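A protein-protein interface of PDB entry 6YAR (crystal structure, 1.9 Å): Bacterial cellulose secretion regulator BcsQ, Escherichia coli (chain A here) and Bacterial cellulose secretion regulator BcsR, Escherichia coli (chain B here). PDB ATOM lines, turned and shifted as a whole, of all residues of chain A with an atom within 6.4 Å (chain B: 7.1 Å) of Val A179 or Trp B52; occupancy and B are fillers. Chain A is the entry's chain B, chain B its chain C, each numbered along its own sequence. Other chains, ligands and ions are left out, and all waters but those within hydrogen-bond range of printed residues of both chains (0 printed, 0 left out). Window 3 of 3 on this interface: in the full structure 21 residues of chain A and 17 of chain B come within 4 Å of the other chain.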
ATOM      1  N   VAL A 149      30.870  21.954  -4.252  1.00  0.00           N
ATOM      2  CA  VAL A 149      29.895  21.136  -3.540  1.00  0.00           C
ATOM      3  C   VAL A 149      29.264  20.167  -4.528  1.00  0.00           C
ATOM      4  O   VAL A 149      28.285  20.501  -5.197  1.00  0.00           O
ATOM      5  CB  VAL A 149      28.823  21.978  -2.844  1.00  0.00           C
ATOM      6  CG1 VAL A 149      27.956  21.064  -1.991  1.00  0.00           C
ATOM      7  CG2 VAL A 149      29.463  23.099  -2.002  1.00  0.00           C
ATOM      8  N   ASP A 150      29.840  18.974  -4.636  1.00  0.00           N
ATOM      9  CA  ASP A 150      29.313  17.922  -5.483  1.00  0.00           C
ATOM     10  C   ASP A 150      29.682  16.586  -4.846  1.00  0.00           C
ATOM     11  O   ASP A 150      30.461  16.519  -3.888  1.00  0.00           O
ATOM     12  CB  ASP A 150      29.821  18.043  -6.935  1.00  0.00           C
ATOM     13  CG  ASP A 150      31.361  18.001  -7.051  1.00  0.00           C
ATOM     14  OD1 ASP A 150      32.021  17.150  -6.412  1.00  0.00           O
ATOM     15  OD2 ASP A 150      31.913  18.827  -7.814  1.00  0.00           O
ATOM     16  N   ALA A 151      29.094  15.513  -5.381  1.00  0.00           N
ATOM     17  CA  ALA A 151      29.298  14.193  -4.793  1.00  0.00           C
ATOM     18  C   ALA A 151      30.757  13.751  -4.884  1.00  0.00           C
ATOM     19  O   ALA A 151      31.253  13.048  -3.992  1.00  0.00           O
ATOM     20  CB  ALA A 151      28.374  13.173  -5.477  1.00  0.00           C
ATOM     21  N   SER A 177      20.608  23.179  -8.155  1.00  0.00           N
ATOM     22  CA  SER A 177      21.044  21.822  -7.828  1.00  0.00           C
ATOM     23  C   SER A 177      20.559  21.427  -6.435  1.00  0.00           C
ATOM     24  O   SER A 177      21.158  21.813  -5.426  1.00  0.00           O
ATOM     25  CB  SER A 177      22.568  21.696  -7.928  1.00  0.00           C
ATOM     26  OG  SER A 177      22.976  20.362  -7.645  1.00  0.00           O
ATOM     27  N   GLN A 178      19.497  20.622  -6.389  1.00  0.00           N
ATOM     28  CA  GLN A 178      19.052  20.036  -5.125  1.00  0.00           C
ATOM     29  C   GLN A 178      20.138  19.179  -4.481  1.00  0.00           C
ATOM     30  O   GLN A 178      20.299  19.189  -3.254  1.00  0.00           O
ATOM     31  CB  GLN A 178      17.797  19.182  -5.345  1.00  0.00           C
ATOM     32  CG  GLN A 178      17.236  18.604  -4.046  1.00  0.00           C
ATOM     33  CD  GLN A 178      16.784  19.685  -3.066  1.00  0.00           C
ATOM     34  OE1 GLN A 178      16.235  20.713  -3.471  1.00  0.00           O
ATOM     35  NE2 GLN A 178      17.029  19.463  -1.774  1.00  0.00           N
ATOM     36  N   VAL A 179      20.865  18.395  -5.274  1.00  0.00           N
ATOM     37  CA  VAL A 179      21.878  17.541  -4.657  1.00  0.00           C
ATOM     38  C   VAL A 179      23.008  18.396  -4.085  1.00  0.00           C
ATOM     39  O   VAL A 179      23.524  18.116  -2.998  1.00  0.00           O
ATOM     40  CB  VAL A 179      22.391  16.464  -5.642  1.00  0.00           C
ATOM     41  CG1 VAL A 179      23.199  17.060  -6.792  1.00  0.00           C
ATOM     42  CG2 VAL A 179      23.228  15.393  -4.898  1.00  0.00           C
ATOM     43  N   GLN A 180      23.407  19.453  -4.792  1.00  0.00           N
ATOM     44  CA  GLN A 180      24.365  20.392  -4.206  1.00  0.00           C
ATOM     45  C   GLN A 180      23.839  20.961  -2.893  1.00  0.00           C
ATOM     46  O   GLN A 180      24.547  20.972  -1.878  1.00  0.00           O
ATOM     47  CB  GLN A 180      24.674  21.525  -5.179  1.00  0.00           C
ATOM     48  CG  GLN A 180      25.605  22.583  -4.585  1.00  0.00           C
ATOM     49  CD  GLN A 180      25.415  23.942  -5.224  1.00  0.00           C
ATOM     50  OE1 GLN A 180      26.232  24.372  -6.038  1.00  0.00           O
ATOM     51  NE2 GLN A 180      24.322  24.618  -4.876  1.00  0.00           N
ATOM     52  N   ASP A 181      22.582  21.420  -2.882  1.00  0.00           N
ATOM     53  CA  ASP A 181      22.053  22.033  -1.664  1.00  0.00           C
ATOM     54  C   ASP A 181      22.009  21.027  -0.517  1.00  0.00           C
ATOM     55  O   ASP A 181      22.290  21.377   0.637  1.00  0.00           O
ATOM     56  CB  ASP A 181      20.656  22.631  -1.920  1.00  0.00           C
ATOM     57  CG  ASP A 181      20.662  23.708  -3.009  1.00  0.00           C
ATOM     58  OD1 ASP A 181      21.740  24.261  -3.320  1.00  0.00           O
ATOM     59  OD2 ASP A 181      19.590  24.010  -3.566  1.00  0.00           O
ATOM     60  N   ASP A 182      21.684  19.765  -0.822  1.00  0.00           N
ATOM     61  CA  ASP A 182      21.666  18.720   0.199  1.00  0.00           C
ATOM     62  C   ASP A 182      23.059  18.466   0.761  1.00  0.00           C
ATOM     63  O   ASP A 182      23.243  18.386   1.981  1.00  0.00           O
ATOM     64  CB  ASP A 182      21.091  17.420  -0.379  1.00  0.00           C
ATOM     65  CG  ASP A 182      19.589  17.494  -0.626  1.00  0.00           C
ATOM     66  OD1 ASP A 182      18.908  18.310   0.032  1.00  0.00           O
ATOM     67  OD2 ASP A 182      19.099  16.724  -1.478  1.00  0.00           O
ATOM     68  N   ILE A 183      24.051  18.296  -0.116  1.00  0.00           N
ATOM     69  CA  ILE A 183      25.418  18.094   0.355  1.00  0.00           C
ATOM     70  C   ILE A 183      25.879  19.302   1.162  1.00  0.00           C
ATOM     71  O   ILE A 183      26.513  19.165   2.219  1.00  0.00           O
ATOM     72  CB  ILE A 183      26.361  17.814  -0.830  1.00  0.00           C
ATOM     73  CG1 ILE A 183      25.978  16.488  -1.507  1.00  0.00           C
ATOM     74  CG2 ILE A 183      27.833  17.820  -0.360  1.00  0.00           C
ATOM     75  CD1 ILE A 183      26.617  16.282  -2.890  1.00  0.00           C
ATOM     76  N   TYR A 184      25.549  20.505   0.683  1.00  0.00           N
ATOM     77  CA  TYR A 184      25.959  21.724   1.377  1.00  0.00           C
ATOM     78  C   TYR A 184      25.396  21.766   2.793  1.00  0.00           C
ATOM     79  O   TYR A 184      26.131  22.015   3.754  1.00  0.00           O
ATOM     80  CB  TYR A 184      25.528  22.954   0.574  1.00  0.00           C
ATOM     81  CG  TYR A 184      25.779  24.273   1.294  1.00  0.00           C
ATOM     82  CD1 TYR A 184      27.074  24.751   1.481  1.00  0.00           C
ATOM     83  CD2 TYR A 184      24.715  25.030   1.786  1.00  0.00           C
ATOM     84  CE1 TYR A 184      27.316  25.950   2.146  1.00  0.00           C
ATOM     85  CE2 TYR A 184      24.946  26.243   2.455  1.00  0.00           C
ATOM     86  CZ  TYR A 184      26.244  26.690   2.626  1.00  0.00           C
ATOM     87  OH  TYR A 184      26.480  27.880   3.284  1.00  0.00           O
ATOM     88  N   ALA B  47      15.893  14.131   5.319  1.00  0.00           N
ATOM     89  CA  ALA B  47      15.311  13.926   3.997  1.00  0.00           C
ATOM     90  C   ALA B  47      16.390  13.753   2.936  1.00  0.00           C
ATOM     91  O   ALA B  47      16.249  12.926   2.024  1.00  0.00           O
ATOM     92  CB  ALA B  47      14.400  15.100   3.640  1.00  0.00           C
ATOM     93  N   ALA B  48      17.472  14.529   3.038  1.00  0.00           N
ATOM     94  CA  ALA B  48      18.574  14.397   2.090  1.00  0.00           C
ATOM     95  C   ALA B  48      19.265  13.050   2.236  1.00  0.00           C
ATOM     96  O   ALA B  48      19.644  12.426   1.236  1.00  0.00           O
ATOM     97  CB  ALA B  48      19.575  15.535   2.282  1.00  0.00           C
ATOM     98  N   LEU B  49      19.452  12.588   3.476  1.00  0.00           N
ATOM     99  CA  LEU B  49      20.063  11.281   3.684  1.00  0.00           C
ATOM    100  C   LEU B  49      19.180  10.168   3.133  1.00  0.00           C
ATOM    101  O   LEU B  49      19.689   9.169   2.612  1.00  0.00           O
ATOM    102  CB  LEU B  49      20.342  11.063   5.173  1.00  0.00           C
ATOM    103  CG  LEU B  49      21.415  11.940   5.828  1.00  0.00           C
ATOM    104  CD1 LEU B  49      21.497  11.641   7.312  1.00  0.00           C
ATOM    105  CD2 LEU B  49      22.782  11.745   5.176  1.00  0.00           C
ATOM    106  N   LYS B  50      17.859  10.333   3.220  1.00  0.00           N
ATOM    107  CA  LYS B  50      16.954   9.356   2.628  1.00  0.00           C
ATOM    108  C   LYS B  50      17.008   9.402   1.107  1.00  0.00           C
ATOM    109  O   LYS B  50      16.930   8.360   0.452  1.00  0.00           O
ATOM    110  CB  LYS B  50      15.526   9.587   3.127  1.00  0.00           C
ATOM    111  CG  LYS B  50      15.335   9.267   4.605  1.00  0.00           C
ATOM    112  CD  LYS B  50      14.002   9.781   5.152  1.00  0.00           C
ATOM    113  CE  LYS B  50      12.817   9.089   4.503  1.00  0.00           C
ATOM    114  NZ  LYS B  50      11.545   9.357   5.240  1.00  0.00           N
ATOM    115  N   ARG B  51      17.130  10.607   0.538  1.00  0.00           N
ATOM    116  CA  ARG B  51      17.206  10.764  -0.911  1.00  0.00           C
ATOM    117  C   ARG B  51      18.469  10.127  -1.476  1.00  0.00           C
ATOM    118  O   ARG B  51      18.417   9.441  -2.503  1.00  0.00           O
ATOM    119  CB  ARG B  51      17.163  12.250  -1.291  1.00  0.00           C
ATOM    120  CG  ARG B  51      15.801  12.931  -1.145  1.00  0.00           C
ATOM    121  CD  ARG B  51      15.727  14.239  -1.947  1.00  0.00           C
ATOM    122  NE  ARG B  51      16.381  15.371  -1.289  1.00  0.00           N
ATOM    123  CZ  ARG B  51      15.790  16.127  -0.371  1.00  0.00           C
ATOM    124  NH1 ARG B  51      14.546  15.866  -0.006  1.00  0.00           N
ATOM    125  NH2 ARG B  51      16.432  17.140   0.189  1.00  0.00           N
ATOM    126  N   TRP B  52      19.610  10.335  -0.818  1.00  0.00           N
ATOM    127  CA  TRP B  52      20.918  10.032  -1.398  1.00  0.00           C
ATOM    128  C   TRP B  52      21.663   8.915  -0.669  1.00  0.00           C
ATOM    129  O   TRP B  52      22.260   9.153   0.392  1.00  0.00           O
ATOM    130  CB  TRP B  52      21.758  11.311  -1.435  1.00  0.00           C
ATOM    131  CG  TRP B  52      21.022  12.430  -2.131  1.00  0.00           C
ATOM    132  CD1 TRP B  52      20.667  13.639  -1.601  1.00  0.00           C
ATOM    133  CD2 TRP B  52      20.512  12.416  -3.472  1.00  0.00           C
ATOM    134  NE1 TRP B  52      19.990  14.385  -2.532  1.00  0.00           N
ATOM    135  CE2 TRP B  52      19.879  13.657  -3.689  1.00  0.00           C
ATOM    136  CE3 TRP B  52      20.531  11.473  -4.511  1.00  0.00           C
ATOM    137  CZ2 TRP B  52      19.271  13.984  -4.902  1.00  0.00           C
ATOM    138  CZ3 TRP B  52      19.936  11.798  -5.713  1.00  0.00           C
ATOM    139  CH2 TRP B  52      19.310  13.046  -5.900  1.00  0.00           C
ATOM    140  N   PRO B  53      21.680   7.693  -1.208  1.00  0.00           N
ATOM    141  CA  PRO B  53      22.405   6.595  -0.539  1.00  0.00           C
ATOM    142  C   PRO B  53      23.885   6.871  -0.302  1.00  0.00           C
ATOM    143  O   PRO B  53      24.438   6.405   0.699  1.00  0.00           O
ATOM    144  CB  PRO B  53      22.203   5.412  -1.499  1.00  0.00           C
ATOM    145  CG  PRO B  53      20.938   5.734  -2.235  1.00  0.00           C
ATOM    146  CD  PRO B  53      20.925   7.232  -2.387  1.00  0.00           C
ATOM    147  N   LEU B  54      24.549   7.607  -1.189  1.00  0.00           N
ATOM    148  CA  LEU B  54      25.951   7.950  -0.955  1.00  0.00           C
ATOM    149  C   LEU B  54      26.140   8.705   0.366  1.00  0.00           C
ATOM    150  O   LEU B  54      27.070   8.412   1.129  1.00  0.00           O
ATOM    151  CB  LEU B  54      26.478   8.773  -2.130  1.00  0.00           C
ATOM    152  CG  LEU B  54      27.966   9.093  -2.149  1.00  0.00           C
ATOM    153  CD1 LEU B  54      28.792   7.829  -2.486  1.00  0.00           C
ATOM    154  CD2 LEU B  54      28.226  10.231  -3.130  1.00  0.00           C
ATOM    155  N   LEU B  55      25.259   9.666   0.664  1.00  0.00           N
ATOM    156  CA  LEU B  55      25.425  10.474   1.875  1.00  0.00           C
ATOM    157  C   LEU B  55      25.078   9.684   3.128  1.00  0.00           C
ATOM    158  O   LEU B  55      25.766   9.801   4.148  1.00  0.00           O
ATOM    159  CB  LEU B  55      24.563  11.733   1.804  1.00  0.00           C
ATOM    160  CG  LEU B  55      24.658  12.580   0.539  1.00  0.00           C
ATOM    161  CD1 LEU B  55      23.719  13.762   0.648  1.00  0.00           C
ATOM    162  CD2 LEU B  55      26.072  13.043   0.305  1.00  0.00           C
ATOM    163  N   ALA B  56      24.006   8.886   3.078  1.00  0.00           N
ATOM    164  CA  ALA B  56      23.669   8.018   4.203  1.00  0.00           C
ATOM    165  C   ALA B  56      24.806   7.057   4.516  1.00  0.00           C
ATOM    166  O   ALA B  56      25.050   6.730   5.682  1.00  0.00           O
ATOM    167  CB  ALA B  56      22.386   7.237   3.904  1.00  0.00           C
ATOM    168  N   GLU B  57      25.517   6.602   3.482  1.00  0.00           N
ATOM    169  CA  GLU B  57      26.577   5.623   3.672  1.00  0.00           C
ATOM    170  C   GLU B  57      27.709   6.188   4.521  1.00  0.00           C
ATOM    171  O   GLU B  57      28.194   5.533   5.450  1.00  0.00           O
ATOM    172  CB  GLU B  57      27.103   5.165   2.313  1.00  0.00           C
ATOM    173  CG  GLU B  57      28.259   4.204   2.418  1.00  0.00           C
ATOM    174  CD  GLU B  57      28.691   3.653   1.078  1.00  0.00           C
ATOM    175  OE1 GLU B  57      28.465   4.323   0.048  1.00  0.00           O
ATOM    176  OE2 GLU B  57      29.264   2.547   1.067  1.00  0.00           O
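NH2 of Arg B51 sits close to NE2 of Gln A178, at 3.1 Å. The guanidinium group of Arg B51 lies within salt-bridge range of the side-chain carboxylate of Asp A182. The indole nitrogen (NE1) of Trp B52 is in hydrogen-bond range of the side-chain carboxylate (OD2) of Asp A182 (2.7 Å).
Of chain B, only Trp B52 (3.96 Å) comes within 4 Å of Val A179. Printed residues of chain A within 4 Å of Trp B52: Val A179 and Asp A182. Of the printed residues of chain A, Leu B54 touches Ala A151 (3.8 Å). Of the printed residues of chain A, Leu B55 touches Ile A183. Of the printed residues of chain B, Ile A183 touches Leu B55. Of the printed residues of chain B, Gln A178 touches Arg B51 (3.1 Å). The nearest residue of chain B that does not touch Val A179 is Leu B55 (5.7 Å).
NE2 of Gln A178 is in hydrogen-bond range of OD1 of Asp A182 (2.8 Å).
Among the printed residues, merely in contact across the chains: Ala A151 with Leu B54, Val A179 with Trp B52, Asp A182 with Ala B48 and Ile A183 with Leu B55.
Of the 11 printed residues of chain A, 5 touch a printed residue of chain B. Printed residues of chain A that touch a printed residue of chain B: Ala A151, Gln A178, Val A179, Asp A182 and Ile A183. Hydrophobic or aromatic side chains of chain A that line the printed part of chain B: Ala A151, Val A179 and Ile A183. Printed residues of chain B that touch a printed residue of chain A: Ala B48, Arg B51, Trp B52, Leu B54 and Leu B55. Hydrophobic or aromatic side chains of chain B within 4 Å of the printed part of chain A: Ala B48, Trp B52, Leu B54 and Leu B55. Along chain B the printed residues that touch a printed residue of chain A span positions 48 to 55. Among the printed residues, Asp or Glu carboxylates within 4 Å of a Lys or Arg side-chain nitrogen of the other chain: Asp A182 with Arg B51.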
